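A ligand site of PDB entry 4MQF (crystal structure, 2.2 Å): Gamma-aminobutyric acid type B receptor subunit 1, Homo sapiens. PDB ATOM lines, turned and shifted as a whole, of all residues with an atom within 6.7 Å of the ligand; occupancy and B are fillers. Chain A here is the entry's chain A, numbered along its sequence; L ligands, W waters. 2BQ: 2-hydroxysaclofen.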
ATOM      1  N   GLY A  17     -17.762 -19.599  -1.041  1.00  0.00           N
ATOM      2  CA  GLY A  17     -18.764 -20.653  -0.902  1.00  0.00           C
ATOM      3  C   GLY A  17     -18.818 -21.590  -2.096  1.00  0.00           C
ATOM      4  O   GLY A  17     -19.057 -22.787  -1.923  1.00  0.00           O
ATOM      5  N   TRP A  18     -18.654 -21.060  -3.311  1.00  0.00           N
ATOM      6  CA  TRP A  18     -18.623 -21.898  -4.512  1.00  0.00           C
ATOM      7  C   TRP A  18     -17.370 -21.528  -5.301  1.00  0.00           C
ATOM      8  O   TRP A  18     -17.359 -20.541  -6.040  1.00  0.00           O
ATOM      9  CB  TRP A  18     -19.893 -21.800  -5.359  1.00  0.00           C
ATOM     10  CG  TRP A  18     -19.825 -22.721  -6.547  1.00  0.00           C
ATOM     11  CD1 TRP A  18     -19.706 -24.086  -6.518  1.00  0.00           C
ATOM     12  CD2 TRP A  18     -19.756 -22.331  -7.933  1.00  0.00           C
ATOM     13  NE1 TRP A  18     -19.621 -24.576  -7.800  1.00  0.00           N
ATOM     14  CE2 TRP A  18     -19.660 -23.518  -8.691  1.00  0.00           C
ATOM     15  CE3 TRP A  18     -19.841 -21.099  -8.601  1.00  0.00           C
ATOM     16  CZ2 TRP A  18     -19.617 -23.503 -10.097  1.00  0.00           C
ATOM     17  CZ3 TRP A  18     -19.744 -21.077  -9.983  1.00  0.00           C
ATOM     18  CH2 TRP A  18     -19.644 -22.272 -10.720  1.00  0.00           C
ATOM     19  N   CYS A  56     -16.138 -15.352  -5.058  1.00  0.00           N
ATOM     20  CA  CYS A  56     -17.538 -15.641  -4.755  1.00  0.00           C
ATOM     21  C   CYS A  56     -18.056 -14.564  -3.765  1.00  0.00           C
ATOM     22  O   CYS A  56     -18.810 -14.859  -2.840  1.00  0.00           O
ATOM     23  CB  CYS A  56     -17.667 -17.049  -4.203  1.00  0.00           C
ATOM     24  SG  CYS A  56     -19.294 -17.776  -4.419  1.00  0.00           S
ATOM     25  N   GLY A  81     -20.036 -15.946 -12.200  1.00  0.00           N
ATOM     26  CA  GLY A  81     -20.318 -17.335 -11.826  1.00  0.00           C
ATOM     27  C   GLY A  81     -21.247 -17.536 -10.640  1.00  0.00           C
ATOM     28  O   GLY A  81     -22.275 -18.192 -10.769  1.00  0.00           O
ATOM     29  N   CYS A  82     -20.876 -17.026  -9.455  1.00  0.00           N
ATOM     30  CA  CYS A  82     -21.644 -17.174  -8.198  1.00  0.00           C
ATOM     31  C   CYS A  82     -22.986 -16.428  -8.309  1.00  0.00           C
ATOM     32  O   CYS A  82     -23.056 -15.379  -8.955  1.00  0.00           O
ATOM     33  CB  CYS A  82     -20.818 -16.702  -6.996  1.00  0.00           C
ATOM     34  SG  CYS A  82     -19.540 -17.899  -6.461  1.00  0.00           S
ATOM     35  N   SER A  83     -24.026 -16.981  -7.680  1.00  0.00           N
ATOM     36  CA  SER A  83     -25.372 -16.377  -7.660  1.00  0.00           C
ATOM     37  C   SER A  83     -25.363 -14.977  -7.070  1.00  0.00           C
ATOM     38  O   SER A  83     -26.046 -14.110  -7.599  1.00  0.00           O
ATOM     39  CB  SER A  83     -26.354 -17.241  -6.902  1.00  0.00           C
ATOM     40  OG  SER A  83     -26.898 -18.249  -7.719  1.00  0.00           O
ATOM     41  N   SER A  84     -24.567 -14.739  -6.008  1.00  0.00           N
ATOM     42  CA  SER A  84     -24.504 -13.425  -5.357  1.00  0.00           C
ATOM     43  C   SER A  84     -23.787 -12.416  -6.210  1.00  0.00           C
ATOM     44  O   SER A  84     -24.153 -11.241  -6.220  1.00  0.00           O
ATOM     45  CB  SER A  84     -23.871 -13.526  -3.962  1.00  0.00           C
ATOM     46  OG  SER A  84     -22.510 -13.950  -4.027  1.00  0.00           O
ATOM     47  N   VAL A  85     -22.772 -12.881  -6.953  1.00  0.00           N
ATOM     48  CA  VAL A  85     -22.016 -12.030  -7.878  1.00  0.00           C
ATOM     49  C   VAL A  85     -22.911 -11.687  -9.094  1.00  0.00           C
ATOM     50  O   VAL A  85     -22.982 -10.522  -9.475  1.00  0.00           O
ATOM     51  CB  VAL A  85     -20.637 -12.650  -8.263  1.00  0.00           C
ATOM     52  CG1 VAL A  85     -19.961 -11.865  -9.398  1.00  0.00           C
ATOM     53  CG2 VAL A  85     -19.726 -12.738  -7.058  1.00  0.00           C
ATOM     54  N   TYR A 103     -22.526 -18.846 -15.855  1.00  0.00           N
ATOM     55  CA  TYR A 103     -22.212 -20.256 -16.064  1.00  0.00           C
ATOM     56  C   TYR A 103     -22.433 -21.095 -14.790  1.00  0.00           C
ATOM     57  O   TYR A 103     -22.385 -22.309 -14.886  1.00  0.00           O
ATOM     58  CB  TYR A 103     -20.775 -20.437 -16.619  1.00  0.00           C
ATOM     59  CG  TYR A 103     -19.747 -19.760 -15.755  1.00  0.00           C
ATOM     60  CD1 TYR A 103     -19.258 -20.387 -14.598  1.00  0.00           C
ATOM     61  CD2 TYR A 103     -19.306 -18.475 -16.036  1.00  0.00           C
ATOM     62  CE1 TYR A 103     -18.361 -19.740 -13.759  1.00  0.00           C
ATOM     63  CE2 TYR A 103     -18.423 -17.812 -15.187  1.00  0.00           C
ATOM     64  CZ  TYR A 103     -17.953 -18.456 -14.057  1.00  0.00           C
ATOM     65  OH  TYR A 103     -17.142 -17.794 -13.201  1.00  0.00           O
ATOM     66  N   GLY A 104     -22.669 -20.468 -13.634  1.00  0.00           N
ATOM     67  CA  GLY A 104     -22.859 -21.215 -12.390  1.00  0.00           C
ATOM     68  C   GLY A 104     -23.991 -20.871 -11.435  1.00  0.00           C
ATOM     69  O   GLY A 104     -24.145 -21.554 -10.431  1.00  0.00           O
ATOM     70  N   SER A 105     -24.823 -19.841 -11.750  1.00  0.00           N
ATOM     71  CA  SER A 105     -25.879 -19.350 -10.844  1.00  0.00           C
ATOM     72  C   SER A 105     -27.163 -20.133 -10.888  1.00  0.00           C
ATOM     73  O   SER A 105     -27.824 -20.213 -11.924  1.00  0.00           O
ATOM     74  CB  SER A 105     -26.142 -17.882 -11.098  1.00  0.00           C
ATOM     75  OG  SER A 105     -24.931 -17.167 -10.880  1.00  0.00           O
ATOM     76  N   SER A 106     -27.524 -20.706  -9.751  1.00  0.00           N
ATOM     77  CA  SER A 106     -28.725 -21.549  -9.608  1.00  0.00           C
ATOM     78  C   SER A 106     -29.881 -20.855  -8.847  1.00  0.00           C
ATOM     79  O   SER A 106     -30.958 -21.432  -8.756  1.00  0.00           O
ATOM     80  CB  SER A 106     -28.344 -22.824  -8.866  1.00  0.00           C
ATOM     81  OG  SER A 106     -27.836 -22.487  -7.581  1.00  0.00           O
ATOM     82  N   SER A 107     -29.642 -19.688  -8.243  1.00  0.00           N
ATOM     83  CA  SER A 107     -30.645 -18.935  -7.462  1.00  0.00           C
ATOM     84  C   SER A 107     -31.965 -18.702  -8.223  1.00  0.00           C
ATOM     85  O   SER A 107     -31.921 -18.097  -9.291  1.00  0.00           O
ATOM     86  CB  SER A 107     -30.057 -17.594  -7.006  1.00  0.00           C
ATOM     87  OG  SER A 107     -30.990 -16.812  -6.275  1.00  0.00           O
ATOM     88  N   HIS A 123     -26.431 -22.395 -16.528  1.00  0.00           N
ATOM     89  CA  HIS A 123     -26.692 -23.165 -15.326  1.00  0.00           C
ATOM     90  C   HIS A 123     -28.214 -23.065 -15.059  1.00  0.00           C
ATOM     91  O   HIS A 123     -28.726 -21.962 -14.979  1.00  0.00           O
ATOM     92  CB  HIS A 123     -25.938 -22.619 -14.102  1.00  0.00           C
ATOM     93  CG  HIS A 123     -25.885 -23.578 -12.937  1.00  0.00           C
ATOM     94  ND1 HIS A 123     -27.036 -23.942 -12.240  1.00  0.00           N
ATOM     95  CD2 HIS A 123     -24.827 -24.159 -12.335  1.00  0.00           C
ATOM     96  CE1 HIS A 123     -26.637 -24.773 -11.291  1.00  0.00           C
ATOM     97  NE2 HIS A 123     -25.320 -24.924 -11.292  1.00  0.00           N
ATOM     98  N   PRO A 124     -28.964 -24.154 -14.842  1.00  0.00           N
ATOM     99  CA  PRO A 124     -30.387 -23.991 -14.559  1.00  0.00           C
ATOM    100  C   PRO A 124     -30.687 -23.405 -13.172  1.00  0.00           C
ATOM    101  O   PRO A 124     -29.799 -23.284 -12.323  1.00  0.00           O
ATOM    102  CB  PRO A 124     -30.935 -25.430 -14.669  1.00  0.00           C
ATOM    103  CG  PRO A 124     -29.910 -26.186 -15.442  1.00  0.00           C
ATOM    104  CD  PRO A 124     -28.612 -25.579 -14.952  1.00  0.00           C
ATOM    105  N   TYR A 203     -29.720 -28.083   3.325  1.00  0.00           N
ATOM    106  CA  TYR A 203     -28.346 -28.409   3.009  1.00  0.00           C
ATOM    107  C   TYR A 203     -27.982 -29.765   3.678  1.00  0.00           C
ATOM    108  O   TYR A 203     -28.799 -30.318   4.407  1.00  0.00           O
ATOM    109  CB  TYR A 203     -27.405 -27.256   3.393  1.00  0.00           C
ATOM    110  CG  TYR A 203     -27.580 -26.072   2.476  1.00  0.00           C
ATOM    111  CD1 TYR A 203     -27.230 -26.139   1.136  1.00  0.00           C
ATOM    112  CD2 TYR A 203     -28.063 -24.859   2.968  1.00  0.00           C
ATOM    113  CE1 TYR A 203     -27.389 -25.052   0.285  1.00  0.00           C
ATOM    114  CE2 TYR A 203     -28.212 -23.758   2.136  1.00  0.00           C
ATOM    115  CZ  TYR A 203     -27.886 -23.853   0.800  1.00  0.00           C
ATOM    116  OH  TYR A 203     -28.082 -22.766  -0.017  1.00  0.00           O
ATOM    117  N   TRP A 231     -27.739 -33.471  -4.767  1.00  0.00           N
ATOM    118  CA  TRP A 231     -26.364 -32.982  -4.872  1.00  0.00           C
ATOM    119  C   TRP A 231     -25.507 -33.219  -3.610  1.00  0.00           C
ATOM    120  O   TRP A 231     -24.357 -32.760  -3.569  1.00  0.00           O
ATOM    121  CB  TRP A 231     -26.236 -31.509  -5.357  1.00  0.00           C
ATOM    122  CG  TRP A 231     -27.231 -30.484  -4.870  1.00  0.00           C
ATOM    123  CD1 TRP A 231     -28.119 -29.806  -5.647  1.00  0.00           C
ATOM    124  CD2 TRP A 231     -27.294 -29.881  -3.568  1.00  0.00           C
ATOM    125  NE1 TRP A 231     -28.770 -28.842  -4.908  1.00  0.00           N
ATOM    126  CE2 TRP A 231     -28.289 -28.869  -3.624  1.00  0.00           C
ATOM    127  CE3 TRP A 231     -26.628 -30.095  -2.349  1.00  0.00           C
ATOM    128  CZ2 TRP A 231     -28.656 -28.107  -2.525  1.00  0.00           C
ATOM    129  CZ3 TRP A 231     -26.979 -29.317  -1.253  1.00  0.00           C
ATOM    130  CH2 TRP A 231     -28.010 -28.370  -1.341  1.00  0.00           C
ATOM    131  N   MET A 265     -25.646 -32.046 -15.798  1.00  0.00           N
ATOM    132  CA  MET A 265     -24.641 -31.055 -16.225  1.00  0.00           C
ATOM    133  C   MET A 265     -23.687 -31.596 -17.318  1.00  0.00           C
ATOM    134  O   MET A 265     -22.927 -30.803 -17.918  1.00  0.00           O
ATOM    135  CB  MET A 265     -23.827 -30.545 -15.034  1.00  0.00           C
ATOM    136  CG  MET A 265     -24.620 -29.677 -14.062  1.00  0.00           C
ATOM    137  SD  MET A 265     -23.519 -29.075 -12.786  1.00  0.00           S
ATOM    138  CE  MET A 265     -24.724 -28.437 -11.533  1.00  0.00           C
ATOM    139  N   GLN A 301     -17.908 -30.251 -11.934  1.00  0.00           N
ATOM    140  CA  GLN A 301     -19.192 -30.709 -12.466  1.00  0.00           C
ATOM    141  C   GLN A 301     -19.921 -29.596 -13.271  1.00  0.00           C
ATOM    142  O   GLN A 301     -20.647 -29.913 -14.223  1.00  0.00           O
ATOM    143  CB  GLN A 301     -20.085 -31.354 -11.380  1.00  0.00           C
ATOM    144  CG  GLN A 301     -20.544 -30.470 -10.221  1.00  0.00           C
ATOM    145  CD  GLN A 301     -21.729 -31.040  -9.454  1.00  0.00           C
ATOM    146  OE1 GLN A 301     -22.413 -31.991  -9.899  1.00  0.00           O
ATOM    147  NE2 GLN A 301     -22.050 -30.419  -8.319  1.00  0.00           N
ATOM    148  N   GLU A 302     -19.672 -28.303 -12.959  1.00  0.00           N
ATOM    149  CA  GLU A 302     -20.308 -27.190 -13.694  1.00  0.00           C
ATOM    150  C   GLU A 302     -19.486 -26.782 -14.905  1.00  0.00           C
ATOM    151  O   GLU A 302     -20.015 -26.113 -15.779  1.00  0.00           O
ATOM    152  CB  GLU A 302     -20.584 -25.968 -12.779  1.00  0.00           C
ATOM    153  CG  GLU A 302     -21.629 -26.209 -11.699  1.00  0.00           C
ATOM    154  CD  GLU A 302     -21.106 -26.873 -10.442  1.00  0.00           C
ATOM    155  OE1 GLU A 302     -19.869 -26.938 -10.290  1.00  0.00           O
ATOM    156  OE2 GLU A 302     -21.924 -27.350  -9.619  1.00  0.00           O
ATOM    157  N   LEU A 305     -20.974 -26.374 -18.394  1.00  0.00           N
ATOM    158  CA  LEU A 305     -21.935 -25.261 -18.531  1.00  0.00           C
ATOM    159  C   LEU A 305     -21.169 -24.018 -18.923  1.00  0.00           C
ATOM    160  O   LEU A 305     -21.653 -23.239 -19.748  1.00  0.00           O
ATOM    161  CB  LEU A 305     -22.721 -25.015 -17.221  1.00  0.00           C
ATOM    162  CG  LEU A 305     -23.373 -26.224 -16.591  1.00  0.00           C
ATOM    163  CD1 LEU A 305     -23.802 -25.926 -15.159  1.00  0.00           C
ATOM    164  CD2 LEU A 305     -24.505 -26.765 -17.455  1.00  0.00           C
HETATM  165 CL   2BQ L   1     -25.219 -26.271  -2.574  1.00  0.00          CL
HETATM  166  C3  2BQ L   1     -24.846 -25.395  -4.068  1.00  0.00           C
HETATM  167  C2  2BQ L   1     -23.558 -24.937  -4.272  1.00  0.00           C
HETATM  168  C4  2BQ L   1     -25.850 -25.169  -5.012  1.00  0.00           C
HETATM  169  C5  2BQ L   1     -25.519 -24.523  -6.212  1.00  0.00           C
HETATM  170  C6  2BQ L   1     -24.219 -24.040  -6.429  1.00  0.00           C
HETATM  171  C1  2BQ L   1     -23.248 -24.244  -5.444  1.00  0.00           C
HETATM  172  C7  2BQ L   1     -23.919 -23.281  -7.685  1.00  0.00           C
HETATM  173  O4  2BQ L   1     -25.120 -23.084  -8.415  1.00  0.00           O
HETATM  174  C8  2BQ L   1     -23.032 -24.128  -8.618  1.00  0.00           C
HETATM  175  N   2BQ L   1     -23.714 -25.368  -8.981  1.00  0.00           N
HETATM  176  C9  2BQ L   1     -23.296 -21.916  -7.406  1.00  0.00           C
HETATM  177  S   2BQ L   1     -24.234 -20.796  -6.568  1.00  0.00           S
HETATM  178  O1  2BQ L   1     -24.618 -21.265  -5.275  1.00  0.00           O
HETATM  179  O2  2BQ L   1     -25.427 -20.511  -7.276  1.00  0.00           O
HETATM  180  O3  2BQ L   1     -23.343 -19.470  -6.424  1.00  0.00           O
HETATM  181  O   HOH W   1     -23.538 -17.403  -4.241  1.00  0.00           O
HETATM  182  O   HOH W   2     -23.365 -22.152  -2.483  1.00  0.00           O
HETATM  183  O   HOH W   3     -24.344 -27.836  -7.152  1.00  0.00           O
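The side-chain hydroxyl (OG) of Ser 83 lies within hydrogen-bond range of an oxygen (O2) of the ligand, at 2.7 Å.
The backbone NH of Ser 106 sits at hydrogen-bond distance from an oxygen (O2) of the ligand (3.2 Å).
The side-chain carboxylate (OE2) of Glu 302 is in salt-bridge range of a nitrogen (N) of the ligand (2.7 Å).
The backbone carbonyl oxygen (O) of Gly 104 lies within hydrogen-bond range of an oxygen (O4) of the ligand, at 2.7 Å.
The backbone NH (N) of Ser 83 sits at hydrogen-bond distance from an oxygen (O3) of the ligand, at 2.9 Å.
A nitrogen (N) of the ligand is in hydrogen-bond range of a ring nitrogen (NE2) of His 123 (2.8 Å).
The side-chain hydroxyl of Ser 106 is in hydrogen-bond range of an oxygen (O4) of the ligand (2.9 Å).
The backbone NH (N) of Ser 106 is in hydrogen-bond range of the side-chain hydroxyl (OG) of Ser 83 (3.2 Å).
The side-chain carboxylate of Glu 302 is in hydrogen-bond range of the side-chain amide nitrogen of Gln 301 (3.3 Å).
The side-chain carboxylate (OE1) of Glu 302 sits at hydrogen-bond distance from the indole nitrogen (NE1) of Trp 18 (3.4 Å).
OG of Ser 105 is in hydrogen-bond range of O of Gly 81, 2.8 Å away.
O of Cys 82 is in hydrogen-bond range of OG of Ser 105, at 3.2 Å.
The backbone NH (N) of Ser 83 lies within hydrogen-bond range of the side-chain hydroxyl (OG) of Ser 105 (3.3 Å).
SG of Cys 56 forms a disulfide with SG of Cys 82 (2.1 Å).
The side-chain sulfur of Cys 56 lies within hydrogen-bond range of the backbone NH of Trp 18 (3.5 Å).
Residues that only touch the ligand: Trp 18, Cys 82, Ser 105, Tyr 203 and Trp 231.
Hydrophobic or aromatic side chains within 4 Å of the ligand: Trp 18, His 123, Tyr 203 and Trp 231.
Ten residues have an atom within 4 Å of the ligand: Trp 18, Cys 82, Ser 83, Gly 104, Ser 105, Ser 106, His 123, Tyr 203, Trp 231 and Glu 302.
Water W1 lies within hydrogen-bond range of O3 of the ligand (3.0 Å), N of Ser 84 (3.4 Å) and N of Ser 83 (3.5 Å).
Water W3 bridges a nitrogen (N) of the ligand (3.1 Å) and the side-chain carboxylate (OE2) of Glu 302 (3.5 Å).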
